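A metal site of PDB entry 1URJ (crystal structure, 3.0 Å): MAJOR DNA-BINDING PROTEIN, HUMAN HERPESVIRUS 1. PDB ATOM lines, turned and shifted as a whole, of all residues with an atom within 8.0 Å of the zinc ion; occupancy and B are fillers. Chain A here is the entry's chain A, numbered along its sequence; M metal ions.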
ATOM      1  N   PRO A 110      15.590  -8.115  16.584  1.00  0.00           N
ATOM      2  CA  PRO A 110      16.782  -8.511  17.342  1.00  0.00           C
ATOM      3  C   PRO A 110      17.803  -9.368  16.619  1.00  0.00           C
ATOM      4  O   PRO A 110      17.479 -10.122  15.693  1.00  0.00           O
ATOM      5  CB  PRO A 110      16.193  -9.238  18.530  1.00  0.00           C
ATOM      6  CG  PRO A 110      15.115 -10.005  17.890  1.00  0.00           C
ATOM      7  CD  PRO A 110      14.458  -8.993  16.937  1.00  0.00           C
ATOM      8  N   ARG A 118      25.442 -15.637  10.024  1.00  0.00           N
ATOM      9  CA  ARG A 118      25.139 -16.971   9.527  1.00  0.00           C
ATOM     10  C   ARG A 118      24.609 -17.005   8.105  1.00  0.00           C
ATOM     11  O   ARG A 118      24.798 -17.983   7.399  1.00  0.00           O
ATOM     12  CB  ARG A 118      24.169 -17.704  10.457  1.00  0.00           C
ATOM     13  CG  ARG A 118      22.745 -17.197  10.442  1.00  0.00           C
ATOM     14  CD  ARG A 118      21.788 -18.341  10.152  1.00  0.00           C
ATOM     15  NE  ARG A 118      20.386 -17.986  10.366  1.00  0.00           N
ATOM     16  CZ  ARG A 118      19.861 -17.714  11.563  1.00  0.00           C
ATOM     17  NH1 ARG A 118      20.628 -17.756  12.647  1.00  0.00           N
ATOM     18  NH2 ARG A 118      18.578 -17.402  11.678  1.00  0.00           N
ATOM     19  N   TYR A 488      -0.602 -15.144  16.530  1.00  0.00           N
ATOM     20  CA  TYR A 488       0.616 -15.890  16.253  1.00  0.00           C
ATOM     21  C   TYR A 488       1.567 -15.870  17.449  1.00  0.00           C
ATOM     22  O   TYR A 488       1.975 -16.925  17.954  1.00  0.00           O
ATOM     23  CB  TYR A 488       1.343 -15.350  15.022  1.00  0.00           C
ATOM     24  CG  TYR A 488       2.710 -15.981  14.850  1.00  0.00           C
ATOM     25  CD1 TYR A 488       2.835 -17.365  14.709  1.00  0.00           C
ATOM     26  CD2 TYR A 488       3.884 -15.227  14.953  1.00  0.00           C
ATOM     27  CE1 TYR A 488       4.077 -17.983  14.683  1.00  0.00           C
ATOM     28  CE2 TYR A 488       5.135 -15.848  14.930  1.00  0.00           C
ATOM     29  CZ  TYR A 488       5.223 -17.234  14.797  1.00  0.00           C
ATOM     30  OH  TYR A 488       6.433 -17.873  14.810  1.00  0.00           O
ATOM     31  N   VAL A 497      10.005 -22.509  18.450  1.00  0.00           N
ATOM     32  CA  VAL A 497       9.971 -21.623  17.284  1.00  0.00           C
ATOM     33  C   VAL A 497      11.157 -21.852  16.352  1.00  0.00           C
ATOM     34  O   VAL A 497      12.286 -22.059  16.814  1.00  0.00           O
ATOM     35  CB  VAL A 497       9.946 -20.147  17.745  1.00  0.00           C
ATOM     36  CG1 VAL A 497      10.115 -19.217  16.556  1.00  0.00           C
ATOM     37  CG2 VAL A 497       8.618 -19.858  18.444  1.00  0.00           C
ATOM     38  N   PRO A 498      10.915 -21.829  15.028  1.00  0.00           N
ATOM     39  CA  PRO A 498      11.943 -22.026  14.004  1.00  0.00           C
ATOM     40  C   PRO A 498      12.809 -20.769  13.807  1.00  0.00           C
ATOM     41  O   PRO A 498      13.008 -20.318  12.683  1.00  0.00           O
ATOM     42  CB  PRO A 498      11.131 -22.322  12.734  1.00  0.00           C
ATOM     43  CG  PRO A 498       9.809 -22.776  13.233  1.00  0.00           C
ATOM     44  CD  PRO A 498       9.573 -21.860  14.422  1.00  0.00           C
ATOM     45  N   CYS A 499      13.305 -20.208  14.908  1.00  0.00           N
ATOM     46  CA  CYS A 499      14.144 -19.011  14.822  1.00  0.00           C
ATOM     47  C   CYS A 499      14.918 -18.803  16.111  1.00  0.00           C
ATOM     48  O   CYS A 499      14.330 -18.722  17.196  1.00  0.00           O
ATOM     49  CB  CYS A 499      13.288 -17.785  14.496  1.00  0.00           C
ATOM     50  SG  CYS A 499      14.178 -16.215  14.580  1.00  0.00           S
ATOM     51  N   ASN A 500      16.250 -18.693  15.998  1.00  0.00           N
ATOM     52  CA  ASN A 500      17.106 -18.511  17.153  1.00  0.00           C
ATOM     53  C   ASN A 500      17.570 -17.067  17.240  1.00  0.00           C
ATOM     54  O   ASN A 500      18.683 -16.790  17.698  1.00  0.00           O
ATOM     55  CB  ASN A 500      18.328 -19.414  17.055  1.00  0.00           C
ATOM     56  CG  ASN A 500      19.255 -18.988  15.933  1.00  0.00           C
ATOM     57  OD1 ASN A 500      18.819 -18.752  14.806  1.00  0.00           O
ATOM     58  ND2 ASN A 500      20.556 -18.899  16.238  1.00  0.00           N
ATOM     59  N   LEU A 501      16.727 -16.146  16.788  1.00  0.00           N
ATOM     60  CA  LEU A 501      17.068 -14.723  16.791  1.00  0.00           C
ATOM     61  C   LEU A 501      16.199 -13.961  17.747  1.00  0.00           C
ATOM     62  O   LEU A 501      16.587 -12.909  18.256  1.00  0.00           O
ATOM     63  CB  LEU A 501      16.866 -14.122  15.398  1.00  0.00           C
ATOM     64  CG  LEU A 501      17.684 -14.651  14.222  1.00  0.00           C
ATOM     65  CD1 LEU A 501      17.076 -14.150  12.928  1.00  0.00           C
ATOM     66  CD2 LEU A 501      19.118 -14.206  14.382  1.00  0.00           C
ATOM     67  N   CYS A 502      15.002 -14.477  17.985  1.00  0.00           N
ATOM     68  CA  CYS A 502      14.070 -13.799  18.874  1.00  0.00           C
ATOM     69  C   CYS A 502      13.560 -14.683  20.000  1.00  0.00           C
ATOM     70  O   CYS A 502      13.888 -15.864  20.124  1.00  0.00           O
ATOM     71  CB  CYS A 502      12.882 -13.309  18.075  1.00  0.00           C
ATOM     72  SG  CYS A 502      11.938 -14.675  17.333  1.00  0.00           S
ATOM     73  N   THR A 503      12.724 -14.072  20.832  1.00  0.00           N
ATOM     74  CA  THR A 503      12.123 -14.740  21.957  1.00  0.00           C
ATOM     75  C   THR A 503      10.690 -14.252  22.044  1.00  0.00           C
ATOM     76  O   THR A 503      10.279 -13.377  21.302  1.00  0.00           O
ATOM     77  CB  THR A 503      12.869 -14.410  23.259  1.00  0.00           C
ATOM     78  OG1 THR A 503      12.435 -15.304  24.284  1.00  0.00           O
ATOM     79  CG2 THR A 503      12.580 -12.973  23.698  1.00  0.00           C
ATOM     80  N   THR A 506      10.063 -10.649  21.959  1.00  0.00           N
ATOM     81  CA  THR A 506      10.510  -9.887  20.795  1.00  0.00           C
ATOM     82  C   THR A 506       9.912 -10.336  19.462  1.00  0.00           C
ATOM     83  O   THR A 506      10.076  -9.656  18.448  1.00  0.00           O
ATOM     84  CB  THR A 506      12.054  -9.875  20.711  1.00  0.00           C
ATOM     85  OG1 THR A 506      12.551 -11.219  20.732  1.00  0.00           O
ATOM     86  CG2 THR A 506      12.652  -9.115  21.886  1.00  0.00           C
ATOM     87  N   ARG A 507       9.207 -11.465  19.457  1.00  0.00           N
ATOM     88  CA  ARG A 507       8.585 -11.987  18.246  1.00  0.00           C
ATOM     89  C   ARG A 507       7.839 -10.929  17.436  1.00  0.00           C
ATOM     90  O   ARG A 507       7.858 -10.966  16.197  1.00  0.00           O
ATOM     91  CB  ARG A 507       7.568 -13.086  18.586  1.00  0.00           C
ATOM     92  CG  ARG A 507       8.133 -14.303  19.242  1.00  0.00           C
ATOM     93  CD  ARG A 507       8.692 -15.302  18.257  1.00  0.00           C
ATOM     94  NE  ARG A 507       9.505 -16.289  18.950  1.00  0.00           N
ATOM     95  CZ  ARG A 507       9.039 -17.111  19.883  1.00  0.00           C
ATOM     96  NH1 ARG A 507       7.753 -17.074  20.236  1.00  0.00           N
ATOM     97  NH2 ARG A 507       9.874 -17.950  20.505  1.00  0.00           N
ATOM     98  N   HIS A 508       7.190  -9.985  18.110  1.00  0.00           N
ATOM     99  CA  HIS A 508       6.434  -8.973  17.377  1.00  0.00           C
ATOM    100  C   HIS A 508       7.265  -8.199  16.344  1.00  0.00           C
ATOM    101  O   HIS A 508       6.736  -7.796  15.297  1.00  0.00           O
ATOM    102  CB  HIS A 508       5.743  -8.009  18.350  1.00  0.00           C
ATOM    103  CG  HIS A 508       6.683  -7.216  19.187  1.00  0.00           C
ATOM    104  ND1 HIS A 508       7.531  -7.795  20.102  1.00  0.00           N
ATOM    105  CD2 HIS A 508       6.909  -5.884  19.265  1.00  0.00           C
ATOM    106  CE1 HIS A 508       8.247  -6.856  20.706  1.00  0.00           C
ATOM    107  NE2 HIS A 508       7.882  -5.677  20.210  1.00  0.00           N
ATOM    108  N   ALA A 509       8.556  -8.014  16.612  1.00  0.00           N
ATOM    109  CA  ALA A 509       9.399  -7.266  15.678  1.00  0.00           C
ATOM    110  C   ALA A 509      10.450  -8.088  14.906  1.00  0.00           C
ATOM    111  O   ALA A 509      11.120  -7.557  14.019  1.00  0.00           O
ATOM    112  CB  ALA A 509      10.086  -6.124  16.412  1.00  0.00           C
ATOM    113  N   CYS A 510      10.571  -9.373  15.228  1.00  0.00           N
ATOM    114  CA  CYS A 510      11.564 -10.223  14.560  1.00  0.00           C
ATOM    115  C   CYS A 510      11.363 -10.407  13.067  1.00  0.00           C
ATOM    116  O   CYS A 510      10.236 -10.535  12.578  1.00  0.00           O
ATOM    117  CB  CYS A 510      11.613 -11.604  15.211  1.00  0.00           C
ATOM    118  SG  CYS A 510      12.839 -12.716  14.474  1.00  0.00           S
ATOM    119  N   VAL A 511      12.469 -10.437  12.341  1.00  0.00           N
ATOM    120  CA  VAL A 511      12.425 -10.634  10.898  1.00  0.00           C
ATOM    121  C   VAL A 511      11.450 -11.752  10.561  1.00  0.00           C
ATOM    122  O   VAL A 511      10.427 -11.523   9.915  1.00  0.00           O
ATOM    123  CB  VAL A 511      13.797 -11.049  10.330  1.00  0.00           C
ATOM    124  CG1 VAL A 511      13.716 -11.121   8.799  1.00  0.00           C
ATOM    125  CG2 VAL A 511      14.877 -10.092  10.776  1.00  0.00           C
ATOM    126  N   HIS A 512      11.775 -12.972  11.003  1.00  0.00           N
ATOM    127  CA  HIS A 512      10.959 -14.142  10.701  1.00  0.00           C
ATOM    128  C   HIS A 512       9.463 -13.874  10.804  1.00  0.00           C
ATOM    129  O   HIS A 512       8.681 -14.350   9.968  1.00  0.00           O
ATOM    130  CB  HIS A 512      11.378 -15.335  11.573  1.00  0.00           C
ATOM    131  CG  HIS A 512      10.471 -15.605  12.731  1.00  0.00           C
ATOM    132  ND1 HIS A 512      10.508 -14.865  13.888  1.00  0.00           N
ATOM    133  CD2 HIS A 512       9.518 -16.550  12.919  1.00  0.00           C
ATOM    134  CE1 HIS A 512       9.618 -15.350  14.748  1.00  0.00           C
ATOM    135  NE2 HIS A 512       9.007 -16.369  14.176  1.00  0.00           N
ATOM    136  N   THR A 513       9.071 -13.099  11.818  1.00  0.00           N
ATOM    137  CA  THR A 513       7.660 -12.775  11.993  1.00  0.00           C
ATOM    138  C   THR A 513       7.211 -11.821  10.899  1.00  0.00           C
ATOM    139  O   THR A 513       6.182 -12.048  10.253  1.00  0.00           O
ATOM    140  CB  THR A 513       7.383 -12.120  13.352  1.00  0.00           C
ATOM    141  OG1 THR A 513       7.755 -13.021  14.400  1.00  0.00           O
ATOM    142  CG2 THR A 513       5.907 -11.792  13.491  1.00  0.00           C
ATOM    143  N   THR A 514       7.984 -10.770  10.695  1.00  0.00           N
ATOM    144  CA  THR A 514       7.630  -9.804   9.662  1.00  0.00           C
ATOM    145  C   THR A 514       7.507 -10.514   8.334  1.00  0.00           C
ATOM    146  O   THR A 514       6.539 -10.281   7.602  1.00  0.00           O
ATOM    147  CB  THR A 514       8.677  -8.697   9.529  1.00  0.00           C
ATOM    148  OG1 THR A 514       8.609  -7.828  10.670  1.00  0.00           O
ATOM    149  CG2 THR A 514       8.430  -7.895   8.248  1.00  0.00           C
ATOM    150  N   MET A 516       6.863 -13.588   7.926  1.00  0.00           N
ATOM    151  CA  MET A 516       5.704 -14.465   7.976  1.00  0.00           C
ATOM    152  C   MET A 516       4.456 -13.687   7.575  1.00  0.00           C
ATOM    153  O   MET A 516       3.627 -14.165   6.807  1.00  0.00           O
ATOM    154  CB  MET A 516       5.513 -15.023   9.383  1.00  0.00           C
ATOM    155  CG  MET A 516       6.271 -16.294   9.655  1.00  0.00           C
ATOM    156  SD  MET A 516       5.803 -16.935  11.256  1.00  0.00           S
ATOM    157  CE  MET A 516       4.119 -17.538  10.883  1.00  0.00           C
HETATM  158 ZN    ZN M   1      12.269 -14.991  15.051  1.00  0.00          ZN
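ND1 of His 512 lies close to OG1 of Thr 513 (3.4 Å).
A ring nitrogen (NE2) of His 512 sits at hydrogen-bond distance from the side-chain hydroxyl (OH) of Tyr 488 (3.0 Å).
N of Leu 501 lies close to SG of Cys 499 (3.4 Å).
The side-chain sulfur (SG) of Cys 502 lies close to the guanidinium group (NE) of Arg 507, 3.3 Å away.
Within 4 Å of the zinc ion: Cys 499, Cys 502, Cys 510 and His 512.
The zinc ion is bound by ND1 of His 512 (2.1 Å), SG of Cys 499 (2.3 Å), SG of Cys 502 (2.3 Å) and SG of Cys 510 (2.4 Å).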
